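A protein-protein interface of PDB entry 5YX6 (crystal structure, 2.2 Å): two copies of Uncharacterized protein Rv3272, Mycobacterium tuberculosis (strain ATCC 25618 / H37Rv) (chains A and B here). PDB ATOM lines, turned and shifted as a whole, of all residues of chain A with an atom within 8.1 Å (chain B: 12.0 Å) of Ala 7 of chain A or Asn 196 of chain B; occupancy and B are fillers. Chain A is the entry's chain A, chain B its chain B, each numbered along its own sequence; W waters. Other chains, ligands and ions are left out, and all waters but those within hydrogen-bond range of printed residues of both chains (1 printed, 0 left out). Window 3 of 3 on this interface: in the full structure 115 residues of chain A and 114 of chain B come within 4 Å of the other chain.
NE2 of His 192 of chain B sits at hydrogen-bond distance from OG of Ser 371 of chain A, at 3.0 Å.
The guanidinium group (NH2) of Arg 195 of chain B lies within hydrogen-bond range of the backbone carbonyl oxygen (O) of Asp 11 of chain A, 2.8 Å away.
The side-chain hydroxyl (OG) of Ser 371 of chain A sits at hydrogen-bond distance from the side-chain carboxylate (OD2) of Asp 200 of chain B (2.7 Å).
The backbone carbonyl oxygen (O) of Lys 8 of chain A sits at hydrogen-bond distance from the side-chain amide nitrogen (ND2) of Asn 196 of chain B (3.2 Å).
NH2 of Arg 195 of chain B lies within hydrogen-bond range of O of Pro 9 of chain A, at 3.0 Å.
The guanidinium group (NH1) of Arg 119 of chain B sits at hydrogen-bond distance from the backbone carbonyl oxygen (O) of Asp 200 of chain B (3.4 Å).
The side-chain amino group (NZ) of Lys 8 of chain A sits at hydrogen-bond distance from the backbone carbonyl oxygen (O) of Arg 373 of chain A (3.3 Å).
A ring nitrogen (ND1) of His 192 of chain B lies within hydrogen-bond range of the side-chain amide nitrogen (ND2) of Asn 196 of chain B (2.9 Å).
NZ of Lys 8 of chain A lies within hydrogen-bond range of O of Asp 33 of chain A (3.0 Å).
OD2 of Asp 11 of chain A is in hydrogen-bond range of N of Lys 8 of chain A, 3.0 Å away.
The backbone carbonyl oxygen (O) of Leu 34 of chain A is in hydrogen-bond range of the backbone NH (N) of Leu 10 of chain A, 2.9 Å away.
Among the printed residues, merely in contact across the chains: Ala 7 of chain A with His 192 of chain B (3.4 Å), Ala 7 of chain A with Asn 196 of chain B (3.9 Å), Lys 8 of chain A with His 192 of chain B (3.99 Å), Pro 9 of chain A with Ala 188 of chain B (3.7 Å), Pro 9 of chain A with His 192 of chain B (3.6 Å), Pro 9 of chain A with Asn 196 of chain B (3.8 Å), Leu 10 of chain A with Leu 191 of chain B (3.5 Å), Leu 10 of chain A with Arg 195 of chain B (3.8 Å), Leu 34 of chain A with Ala 188 of chain B (3.95 Å), Glu 194 of chain A with Glu 194 of chain B (3.7 Å), Glu 194 of chain A with Arg 195 of chain B (3.97 Å), Ser 371 of chain A with Val 198 of chain B (3.6 Å), Phe 372 of chain A with His 192 of chain B (3.9 Å) and Phe 372 of chain A with Asp 200 of chain B (3.9 Å).
Of chain A, only Ala 7, Lys 8 and Pro 9 come within 4 Å of Asn 196 of chain B.
No residue of chain B comes within 4 Å of Asn 5 of chain A.
No residue of chain B comes within 4 Å of Pro 6 of chain A.
Of the printed residues of chain B, Ser 371 of chain A touches His 192 (3.0 Å), Val 198 (3.6 Å) and Asp 200 (2.7 Å).
No residue of chain A comes within 4 Å of Gly 197 of chain B.
Of the printed residues of chain B, Leu 10 of chain A touches Leu 191 and Arg 195.
Of the printed residues of chain A, Val 198 of chain B touches Ser 371.
Printed residues of chain A within 4 Å of Arg 195 of chain B: Pro 9 (3.0 Å), Leu 10 (3.8 Å), Asp 11 (2.8 Å) and Glu 194 (3.97 Å).
The nearest residue of chain B that does not touch Ala 7 of chain A is Val 198 of chain B (5.7 Å).
Hydrophobic or aromatic side chains of chain B that line the printed part of chain A: Ala 188, Leu 191, His 192 and Val 198.
Printed residues of chain A that touch a printed residue of chain B: Ala 7, Lys 8, Pro 9, Leu 10, Asp 11, Leu 34, Glu 194, Ser 371 and Phe 372.
Hydrophobic or aromatic side chains of chain A that line the printed part of chain B: Ala 7, Pro 9, Leu 10, Leu 34 and Phe 372.
Glu 194 of chain B touches its own counterpart, Glu 194 of chain A.
Position printed for both chains: 194.
Of the 19 pairs that touch across the chains among the printed residues, 1 has its exchanged pair printed and touching as well.
Water W1 lies within hydrogen-bond range of O of Ala 7 of chain A (2.7 Å), O of Ser 371 of chain A (2.9 Å) and NE2 of His 192 of chain B (3.3 Å).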
ATOM      1  N   ASN A   5      26.247  -8.343  14.710  1.00  0.00           N
ATOM      2  CA  ASN A   5      25.226  -8.184  13.678  1.00  0.00           C
ATOM      3  C   ASN A   5      23.782  -8.440  14.159  1.00  0.00           C
ATOM      4  O   ASN A   5      22.902  -7.620  13.878  1.00  0.00           O
ATOM      5  CB  ASN A   5      25.550  -9.084  12.477  1.00  0.00           C
ATOM      6  N   PRO A   6      23.519  -9.574  14.857  1.00  0.00           N
ATOM      7  CA  PRO A   6      22.131  -9.771  15.305  1.00  0.00           C
ATOM      8  C   PRO A   6      21.730  -8.855  16.462  1.00  0.00           C
ATOM      9  O   PRO A   6      22.578  -8.427  17.244  1.00  0.00           O
ATOM     10  CB  PRO A   6      22.112 -11.230  15.755  1.00  0.00           C
ATOM     11  CG  PRO A   6      23.519 -11.515  16.145  1.00  0.00           C
ATOM     12  CD  PRO A   6      24.362 -10.741  15.184  1.00  0.00           C
ATOM     13  N   ALA A   7      20.434  -8.599  16.589  1.00  0.00           N
ATOM     14  CA  ALA A   7      19.918  -7.735  17.644  1.00  0.00           C
ATOM     15  C   ALA A   7      20.245  -8.250  19.044  1.00  0.00           C
ATOM     16  O   ALA A   7      20.243  -9.455  19.294  1.00  0.00           O
ATOM     17  CB  ALA A   7      18.420  -7.574  17.489  1.00  0.00           C
ATOM     18  N   LYS A   8      20.514  -7.325  19.957  1.00  0.00           N
ATOM     19  CA  LYS A   8      20.741  -7.675  21.355  1.00  0.00           C
ATOM     20  C   LYS A   8      19.651  -7.022  22.193  1.00  0.00           C
ATOM     21  O   LYS A   8      19.138  -5.964  21.817  1.00  0.00           O
ATOM     22  CB  LYS A   8      22.125  -7.220  21.820  1.00  0.00           C
ATOM     23  CG  LYS A   8      23.271  -7.978  21.212  1.00  0.00           C
ATOM     24  CD  LYS A   8      24.527  -7.662  21.975  1.00  0.00           C
ATOM     25  CE  LYS A   8      25.671  -8.575  21.577  1.00  0.00           C
ATOM     26  NZ  LYS A   8      26.827  -8.400  22.505  1.00  0.00           N
ATOM     27  N   PRO A   9      19.312  -7.630  23.342  1.00  0.00           N
ATOM     28  CA  PRO A   9      18.163  -7.175  24.137  1.00  0.00           C
ATOM     29  C   PRO A   9      18.139  -5.676  24.450  1.00  0.00           C
ATOM     30  O   PRO A   9      17.054  -5.106  24.448  1.00  0.00           O
ATOM     31  CB  PRO A   9      18.295  -7.989  25.428  1.00  0.00           C
ATOM     32  CG  PRO A   9      18.970  -9.249  24.994  1.00  0.00           C
ATOM     33  CD  PRO A   9      19.926  -8.843  23.905  1.00  0.00           C
ATOM     34  N   LEU A  10      19.300  -5.061  24.675  1.00  0.00           N
ATOM     35  CA  LEU A  10      19.381  -3.685  25.150  1.00  0.00           C
ATOM     36  C   LEU A  10      19.904  -2.665  24.134  1.00  0.00           C
ATOM     37  O   LEU A  10      20.344  -1.582  24.526  1.00  0.00           O
ATOM     38  CB  LEU A  10      20.266  -3.620  26.403  1.00  0.00           C
ATOM     39  CG  LEU A  10      19.837  -4.513  27.563  1.00  0.00           C
ATOM     40  CD1 LEU A  10      20.663  -4.251  28.801  1.00  0.00           C
ATOM     41  CD2 LEU A  10      18.363  -4.285  27.843  1.00  0.00           C
ATOM     42  N   ASP A  11      19.894  -3.011  22.848  1.00  0.00           N
ATOM     43  CA  ASP A  11      20.233  -2.045  21.793  1.00  0.00           C
ATOM     44  C   ASP A  11      19.454  -0.747  21.965  1.00  0.00           C
ATOM     45  O   ASP A  11      18.241  -0.764  22.189  1.00  0.00           O
ATOM     46  CB  ASP A  11      19.952  -2.606  20.393  1.00  0.00           C
ATOM     47  CG  ASP A  11      20.906  -3.721  20.004  1.00  0.00           C
ATOM     48  OD1 ASP A  11      22.007  -3.801  20.602  1.00  0.00           O
ATOM     49  OD2 ASP A  11      20.570  -4.493  19.072  1.00  0.00           O
ATOM     50  N   GLY A  12      20.159   0.374  21.892  1.00  0.00           N
ATOM     51  CA  GLY A  12      19.517   1.667  21.975  1.00  0.00           C
ATOM     52  C   GLY A  12      19.449   2.246  23.376  1.00  0.00           C
ATOM     53  O   GLY A  12      19.193   3.437  23.528  1.00  0.00           O
ATOM     54  N   ASP A  33      27.280  -6.600  27.625  1.00  0.00           N
ATOM     55  CA  ASP A  33      27.163  -7.874  26.920  1.00  0.00           C
ATOM     56  C   ASP A  33      25.780  -8.021  26.278  1.00  0.00           C
ATOM     57  O   ASP A  33      25.624  -8.670  25.243  1.00  0.00           O
ATOM     58  CB  ASP A  33      27.416  -9.044  27.873  1.00  0.00           C
ATOM     59  CG  ASP A  33      28.846  -9.053  28.448  1.00  0.00           C
ATOM     60  OD1 ASP A  33      29.746  -8.391  27.870  1.00  0.00           O
ATOM     61  OD2 ASP A  33      29.072  -9.757  29.468  1.00  0.00           O
ATOM     62  N   LEU A  34      24.781  -7.405  26.897  1.00  0.00           N
ATOM     63  CA  LEU A  34      23.417  -7.461  26.399  1.00  0.00           C
ATOM     64  C   LEU A  34      23.109  -6.314  25.424  1.00  0.00           C
ATOM     65  O   LEU A  34      21.971  -6.157  24.983  1.00  0.00           O
ATOM     66  CB  LEU A  34      22.441  -7.454  27.577  1.00  0.00           C
ATOM     67  CG  LEU A  34      22.598  -8.674  28.497  1.00  0.00           C
ATOM     68  CD1 LEU A  34      21.726  -8.551  29.743  1.00  0.00           C
ATOM     69  CD2 LEU A  34      22.305  -9.984  27.755  1.00  0.00           C
ATOM     70  N   GLY A  35      24.124  -5.525  25.082  1.00  0.00           N
ATOM     71  CA  GLY A  35      24.005  -4.556  24.006  1.00  0.00           C
ATOM     72  C   GLY A  35      23.836  -3.086  24.371  1.00  0.00           C
ATOM     73  O   GLY A  35      23.728  -2.228  23.489  1.00  0.00           O
ATOM     74  N   GLU A 194       9.111  -0.491  30.148  1.00  0.00           N
ATOM     75  CA  GLU A 194       8.673  -0.881  28.818  1.00  0.00           C
ATOM     76  C   GLU A 194       7.190  -1.223  28.781  1.00  0.00           C
ATOM     77  O   GLU A 194       6.469  -0.781  27.889  1.00  0.00           O
ATOM     78  CB  GLU A 194       9.496  -2.075  28.333  1.00  0.00           C
ATOM     79  CG  GLU A 194       9.485  -2.326  26.824  1.00  0.00           C
ATOM     80  CD  GLU A 194      10.182  -1.258  25.992  1.00  0.00           C
ATOM     81  OE1 GLU A 194      11.076  -0.541  26.518  1.00  0.00           O
ATOM     82  OE2 GLU A 194       9.840  -1.166  24.788  1.00  0.00           O
ATOM     83  N   SER A 371      20.060 -16.664  20.384  1.00  0.00           N
ATOM     84  CA  SER A 371      19.884 -15.733  19.267  1.00  0.00           C
ATOM     85  C   SER A 371      20.954 -14.637  19.163  1.00  0.00           C
ATOM     86  O   SER A 371      20.977 -13.876  18.192  1.00  0.00           O
ATOM     87  CB  SER A 371      18.508 -15.078  19.362  1.00  0.00           C
ATOM     88  OG  SER A 371      18.518 -14.051  20.343  1.00  0.00           O
ATOM     89  N   PHE A 372      21.842 -14.564  20.151  1.00  0.00           N
ATOM     90  CA  PHE A 372      22.946 -13.602  20.124  1.00  0.00           C
ATOM     91  C   PHE A 372      24.029 -14.068  21.088  1.00  0.00           C
ATOM     92  O   PHE A 372      23.765 -14.876  21.985  1.00  0.00           O
ATOM     93  CB  PHE A 372      22.472 -12.187  20.507  1.00  0.00           C
ATOM     94  CG  PHE A 372      22.096 -12.048  21.958  1.00  0.00           C
ATOM     95  CD1 PHE A 372      20.831 -12.402  22.399  1.00  0.00           C
ATOM     96  CD2 PHE A 372      23.014 -11.570  22.884  1.00  0.00           C
ATOM     97  CE1 PHE A 372      20.492 -12.293  23.735  1.00  0.00           C
ATOM     98  CE2 PHE A 372      22.682 -11.457  24.219  1.00  0.00           C
ATOM     99  CZ  PHE A 372      21.420 -11.821  24.648  1.00  0.00           C
ATOM    100  N   ARG A 373      25.245 -13.557  20.907  1.00  0.00           N
ATOM    101  CA  ARG A 373      26.351 -13.880  21.807  1.00  0.00           C
ATOM    102  C   ARG A 373      26.517 -12.811  22.890  1.00  0.00           C
ATOM    103  O   ARG A 373      26.825 -11.654  22.587  1.00  0.00           O
ATOM    104  CB  ARG A 373      27.650 -14.049  21.014  1.00  0.00           C
ATOM    105  N   PHE B  13       2.295 -12.007  32.750  1.00  0.00           N
ATOM    106  CA  PHE B  13       3.171 -13.075  32.266  1.00  0.00           C
ATOM    107  C   PHE B  13       2.927 -14.362  33.035  1.00  0.00           C
ATOM    108  O   PHE B  13       2.705 -14.342  34.243  1.00  0.00           O
ATOM    109  CB  PHE B  13       4.650 -12.687  32.380  1.00  0.00           C
ATOM    110  CG  PHE B  13       5.094 -11.648  31.386  1.00  0.00           C
ATOM    111  CD1 PHE B  13       4.474 -11.530  30.157  1.00  0.00           C
ATOM    112  CD2 PHE B  13       6.154 -10.807  31.671  1.00  0.00           C
ATOM    113  CE1 PHE B  13       4.892 -10.578  29.239  1.00  0.00           C
ATOM    114  CE2 PHE B  13       6.573  -9.856  30.752  1.00  0.00           C
ATOM    115  CZ  PHE B  13       5.943  -9.748  29.535  1.00  0.00           C
ATOM    116  N   ARG B 119       8.494 -24.861  21.441  1.00  0.00           N
ATOM    117  CA  ARG B 119       8.623 -23.657  20.621  1.00  0.00           C
ATOM    118  C   ARG B 119       8.046 -23.854  19.224  1.00  0.00           C
ATOM    119  O   ARG B 119       7.751 -22.881  18.533  1.00  0.00           O
ATOM    120  CB  ARG B 119      10.083 -23.209  20.545  1.00  0.00           C
ATOM    121  CG  ARG B 119      10.587 -22.558  21.838  1.00  0.00           C
ATOM    122  CD  ARG B 119      12.108 -22.622  21.940  1.00  0.00           C
ATOM    123  NE  ARG B 119      12.803 -21.882  20.887  1.00  0.00           N
ATOM    124  CZ  ARG B 119      13.032 -20.574  20.910  1.00  0.00           C
ATOM    125  NH1 ARG B 119      12.626 -19.846  21.944  1.00  0.00           N
ATOM    126  NH2 ARG B 119      13.677 -19.996  19.904  1.00  0.00           N
ATOM    127  N   PRO B 123       5.696 -19.975  19.308  1.00  0.00           N
ATOM    128  CA  PRO B 123       6.823 -19.180  18.810  1.00  0.00           C
ATOM    129  C   PRO B 123       7.184 -17.979  19.684  1.00  0.00           C
ATOM    130  O   PRO B 123       8.182 -17.320  19.400  1.00  0.00           O
ATOM    131  CB  PRO B 123       6.338 -18.714  17.433  1.00  0.00           C
ATOM    132  CG  PRO B 123       4.854 -18.816  17.490  1.00  0.00           C
ATOM    133  CD  PRO B 123       4.586 -20.010  18.340  1.00  0.00           C
ATOM    134  N   ASN B 124       6.369 -17.676  20.690  1.00  0.00           N
ATOM    135  CA  ASN B 124       6.647 -16.565  21.595  1.00  0.00           C
ATOM    136  C   ASN B 124       7.206 -17.059  22.934  1.00  0.00           C
ATOM    137  O   ASN B 124       7.479 -16.270  23.834  1.00  0.00           O
ATOM    138  CB  ASN B 124       5.377 -15.747  21.839  1.00  0.00           C
ATOM    139  CG  ASN B 124       4.924 -14.982  20.604  1.00  0.00           C
ATOM    140  OD1 ASN B 124       5.729 -14.609  19.747  1.00  0.00           O
ATOM    141  ND2 ASN B 124       3.620 -14.765  20.500  1.00  0.00           N
ATOM    142  N   ILE B 126       9.618 -18.367  25.765  1.00  0.00           N
ATOM    143  CA  ILE B 126      11.002 -18.319  26.204  1.00  0.00           C
ATOM    144  C   ILE B 126      11.312 -19.571  26.995  1.00  0.00           C
ATOM    145  O   ILE B 126      10.591 -19.933  27.921  1.00  0.00           O
ATOM    146  CB  ILE B 126      11.276 -17.049  27.039  1.00  0.00           C
ATOM    147  CG1 ILE B 126      11.251 -15.836  26.115  1.00  0.00           C
ATOM    148  CG2 ILE B 126      12.603 -17.137  27.771  1.00  0.00           C
ATOM    149  CD1 ILE B 126      10.882 -14.567  26.807  1.00  0.00           C
ATOM    150  N   ALA B 185      18.786 -13.673  33.438  1.00  0.00           N
ATOM    151  CA  ALA B 185      18.743 -14.081  32.036  1.00  0.00           C
ATOM    152  C   ALA B 185      17.304 -14.203  31.507  1.00  0.00           C
ATOM    153  O   ALA B 185      17.034 -13.916  30.345  1.00  0.00           O
ATOM    154  CB  ALA B 185      19.477 -15.384  31.859  1.00  0.00           C
ATOM    155  N   VAL B 186      16.382 -14.643  32.356  1.00  0.00           N
ATOM    156  CA  VAL B 186      14.972 -14.665  31.983  1.00  0.00           C
ATOM    157  C   VAL B 186      14.468 -13.225  31.766  1.00  0.00           C
ATOM    158  O   VAL B 186      13.765 -12.944  30.797  1.00  0.00           O
ATOM    159  CB  VAL B 186      14.126 -15.400  33.045  1.00  0.00           C
ATOM    160  CG1 VAL B 186      12.643 -15.126  32.844  1.00  0.00           C
ATOM    161  CG2 VAL B 186      14.409 -16.907  32.974  1.00  0.00           C
ATOM    162  N   LEU B 187      14.854 -12.313  32.655  1.00  0.00           N
ATOM    163  CA  LEU B 187      14.487 -10.906  32.515  1.00  0.00           C
ATOM    164  C   LEU B 187      15.018 -10.310  31.208  1.00  0.00           C
ATOM    165  O   LEU B 187      14.309  -9.587  30.504  1.00  0.00           O
ATOM    166  CB  LEU B 187      15.027 -10.104  33.699  1.00  0.00           C
ATOM    167  CG  LEU B 187      14.136  -9.734  34.888  1.00  0.00           C
ATOM    168  CD1 LEU B 187      12.739 -10.311  34.779  1.00  0.00           C
ATOM    169  CD2 LEU B 187      14.788 -10.084  36.231  1.00  0.00           C
ATOM    170  N   ALA B 188      16.274 -10.612  30.889  1.00  0.00           N
ATOM    171  CA  ALA B 188      16.879 -10.155  29.639  1.00  0.00           C
ATOM    172  C   ALA B 188      16.109 -10.684  28.430  1.00  0.00           C
ATOM    173  O   ALA B 188      15.877  -9.955  27.468  1.00  0.00           O
ATOM    174  CB  ALA B 188      18.336 -10.578  29.566  1.00  0.00           C
ATOM    175  N   ALA B 189      15.737 -11.960  28.482  1.00  0.00           N
ATOM    176  CA  ALA B 189      14.985 -12.603  27.404  1.00  0.00           C
ATOM    177  C   ALA B 189      13.625 -11.946  27.196  1.00  0.00           C
ATOM    178  O   ALA B 189      13.206 -11.710  26.067  1.00  0.00           O
ATOM    179  CB  ALA B 189      14.812 -14.097  27.696  1.00  0.00           C
ATOM    180  N   LEU B 190      12.942 -11.646  28.293  1.00  0.00           N
ATOM    181  CA  LEU B 190      11.654 -10.957  28.240  1.00  0.00           C
ATOM    182  C   LEU B 190      11.764  -9.578  27.571  1.00  0.00           C
ATOM    183  O   LEU B 190      10.863  -9.146  26.853  1.00  0.00           O
ATOM    184  CB  LEU B 190      11.098 -10.807  29.656  1.00  0.00           C
ATOM    185  CG  LEU B 190      10.494 -12.046  30.321  1.00  0.00           C
ATOM    186  CD1 LEU B 190      10.003 -11.753  31.746  1.00  0.00           C
ATOM    187  CD2 LEU B 190       9.402 -12.676  29.442  1.00  0.00           C
ATOM    188  N   LEU B 191      12.876  -8.893  27.811  1.00  0.00           N
ATOM    189  CA  LEU B 191      13.091  -7.584  27.223  1.00  0.00           C
ATOM    190  C   LEU B 191      13.393  -7.763  25.733  1.00  0.00           C
ATOM    191  O   LEU B 191      12.947  -6.979  24.899  1.00  0.00           O
ATOM    192  CB  LEU B 191      14.214  -6.856  27.965  1.00  0.00           C
ATOM    193  CG  LEU B 191      14.337  -5.334  28.065  1.00  0.00           C
ATOM    194  CD1 LEU B 191      13.011  -4.623  28.286  1.00  0.00           C
ATOM    195  CD2 LEU B 191      15.256  -5.039  29.231  1.00  0.00           C
ATOM    196  N   HIS B 192      14.141  -8.813  25.410  1.00  0.00           N
ATOM    197  CA  HIS B 192      14.499  -9.158  24.030  1.00  0.00           C
ATOM    198  C   HIS B 192      13.254  -9.386  23.170  1.00  0.00           C
ATOM    199  O   HIS B 192      13.143  -8.891  22.058  1.00  0.00           O
ATOM    200  CB  HIS B 192      15.368 -10.423  24.013  1.00  0.00           C
ATOM    201  CG  HIS B 192      16.164 -10.612  22.759  1.00  0.00           C
ATOM    202  ND1 HIS B 192      16.582  -9.561  21.973  1.00  0.00           N
ATOM    203  CD2 HIS B 192      16.656 -11.731  22.176  1.00  0.00           C
ATOM    204  CE1 HIS B 192      17.281 -10.025  20.953  1.00  0.00           C
ATOM    205  NE2 HIS B 192      17.341 -11.340  21.052  1.00  0.00           N
ATOM    206  N   ARG B 193      12.340 -10.175  23.709  1.00  0.00           N
ATOM    207  CA  ARG B 193      11.077 -10.501  23.074  1.00  0.00           C
ATOM    208  C   ARG B 193      10.228  -9.241  22.924  1.00  0.00           C
ATOM    209  O   ARG B 193       9.593  -9.007  21.886  1.00  0.00           O
ATOM    210  CB  ARG B 193      10.381 -11.569  23.909  1.00  0.00           C
ATOM    211  CG  ARG B 193       9.183 -12.254  23.298  1.00  0.00           C
ATOM    212  CD  ARG B 193       8.062 -12.047  24.276  1.00  0.00           C
ATOM    213  NE  ARG B 193       7.424 -13.278  24.695  1.00  0.00           N
ATOM    214  CZ  ARG B 193       6.613 -13.365  25.744  1.00  0.00           C
ATOM    215  NH1 ARG B 193       6.059 -14.525  26.050  1.00  0.00           N
ATOM    216  NH2 ARG B 193       6.380 -12.302  26.503  1.00  0.00           N
ATOM    217  N   GLU B 194      10.232  -8.429  23.977  1.00  0.00           N
ATOM    218  CA  GLU B 194       9.458  -7.197  24.026  1.00  0.00           C
ATOM    219  C   GLU B 194       9.902  -6.171  22.981  1.00  0.00           C
ATOM    220  O   GLU B 194       9.073  -5.556  22.322  1.00  0.00           O
ATOM    221  CB  GLU B 194       9.568  -6.590  25.423  1.00  0.00           C
ATOM    222  CG  GLU B 194       8.430  -5.696  25.816  1.00  0.00           C
ATOM    223  CD  GLU B 194       7.124  -6.456  25.992  1.00  0.00           C
ATOM    224  OE1 GLU B 194       7.165  -7.677  26.269  1.00  0.00           O
ATOM    225  OE2 GLU B 194       6.052  -5.829  25.851  1.00  0.00           O
ATOM    226  N   ARG B 195      11.210  -6.000  22.824  1.00  0.00           N
ATOM    227  CA  ARG B 195      11.756  -4.957  21.952  1.00  0.00           C
ATOM    228  C   ARG B 195      12.160  -5.426  20.549  1.00  0.00           C
ATOM    229  O   ARG B 195      12.128  -4.648  19.600  1.00  0.00           O
ATOM    230  CB  ARG B 195      12.964  -4.310  22.621  1.00  0.00           C
ATOM    231  CG  ARG B 195      12.675  -3.838  24.027  1.00  0.00           C
ATOM    232  CD  ARG B 195      13.828  -3.076  24.616  1.00  0.00           C
ATOM    233  NE  ARG B 195      14.110  -1.835  23.907  1.00  0.00           N
ATOM    234  CZ  ARG B 195      15.257  -1.565  23.288  1.00  0.00           C
ATOM    235  NH1 ARG B 195      15.413  -0.388  22.688  1.00  0.00           N
ATOM    236  NH2 ARG B 195      16.244  -2.460  23.268  1.00  0.00           N
ATOM    237  N   ASN B 196      12.590  -6.675  20.422  1.00  0.00           N
ATOM    238  CA  ASN B 196      13.126  -7.151  19.150  1.00  0.00           C
ATOM    239  C   ASN B 196      12.286  -8.274  18.541  1.00  0.00           C
ATOM    240  O   ASN B 196      12.542  -8.720  17.423  1.00  0.00           O
ATOM    241  CB  ASN B 196      14.568  -7.640  19.330  1.00  0.00           C
ATOM    242  CG  ASN B 196      15.479  -6.568  19.871  1.00  0.00           C
ATOM    243  OD1 ASN B 196      15.474  -5.431  19.402  1.00  0.00           O
ATOM    244  ND2 ASN B 196      16.284  -6.930  20.858  1.00  0.00           N
ATOM    245  N   GLY B 197      11.297  -8.742  19.294  1.00  0.00           N
ATOM    246  CA  GLY B 197      10.411  -9.787  18.820  1.00  0.00           C
ATOM    247  C   GLY B 197      11.027 -11.172  18.825  1.00  0.00           C
ATOM    248  O   GLY B 197      10.488 -12.092  18.218  1.00  0.00           O
ATOM    249  N   VAL B 198      12.135 -11.339  19.539  1.00  0.00           N
ATOM    250  CA  VAL B 198      12.792 -12.640  19.608  1.00  0.00           C
ATOM    251  C   VAL B 198      12.502 -13.372  20.909  1.00  0.00           C
ATOM    252  O   VAL B 198      12.751 -12.850  21.989  1.00  0.00           O
ATOM    253  CB  VAL B 198      14.326 -12.509  19.460  1.00  0.00           C
ATOM    254  CG1 VAL B 198      15.004 -13.876  19.595  1.00  0.00           C
ATOM    255  CG2 VAL B 198      14.679 -11.863  18.133  1.00  0.00           C
ATOM    256  N   ALA B 199      11.998 -14.598  20.794  1.00  0.00           N
ATOM    257  CA  ALA B 199      11.751 -15.450  21.950  1.00  0.00           C
ATOM    258  C   ALA B 199      12.861 -16.502  22.004  1.00  0.00           C
ATOM    259  O   ALA B 199      12.902 -17.420  21.180  1.00  0.00           O
ATOM    260  CB  ALA B 199      10.370 -16.104  21.861  1.00  0.00           C
ATOM    261  N   ASP B 200      13.744 -16.366  22.989  1.00  0.00           N
ATOM    262  CA  ASP B 200      15.039 -17.047  22.994  1.00  0.00           C
ATOM    263  C   ASP B 200      15.099 -18.323  23.819  1.00  0.00           C
ATOM    264  O   ASP B 200      14.220 -18.600  24.638  1.00  0.00           O
ATOM    265  CB  ASP B 200      16.110 -16.079  23.504  1.00  0.00           C
ATOM    266  CG  ASP B 200      17.408 -16.200  22.743  1.00  0.00           C
ATOM    267  OD1 ASP B 200      17.649 -17.265  22.138  1.00  0.00           O
ATOM    268  OD2 ASP B 200      18.166 -15.210  22.704  1.00  0.00           O
ATOM    269  N   VAL B 201      16.161 -19.091  23.600  1.00  0.00           N
ATOM    270  CA  VAL B 201      16.508 -20.194  24.487  1.00  0.00           C
ATOM    271  C   VAL B 201      17.644 -19.700  25.378  1.00  0.00           C
ATOM    272  O   VAL B 201      18.652 -19.186  24.897  1.00  0.00           O
ATOM    273  CB  VAL B 201      16.921 -21.473  23.720  1.00  0.00           C
ATOM    274  CG1 VAL B 201      17.259 -22.597  24.697  1.00  0.00           C
ATOM    275  CG2 VAL B 201      15.802 -21.918  22.771  1.00  0.00           C
ATOM    276  N   VAL B 202      17.443 -19.814  26.681  1.00  0.00           N
ATOM    277  CA  VAL B 202      18.372 -19.263  27.647  1.00  0.00           C
ATOM    278  C   VAL B 202      19.026 -20.404  28.411  1.00  0.00           C
ATOM    279  O   VAL B 202      18.343 -21.349  28.810  1.00  0.00           O
ATOM    280  CB  VAL B 202      17.654 -18.302  28.626  1.00  0.00           C
ATOM    281  CG1 VAL B 202      18.471 -18.103  29.887  1.00  0.00           C
ATOM    282  CG2 VAL B 202      17.378 -16.983  27.959  1.00  0.00           C
HETATM  283  O   HOH W   1      19.046 -11.686  18.302  1.00  0.00           O
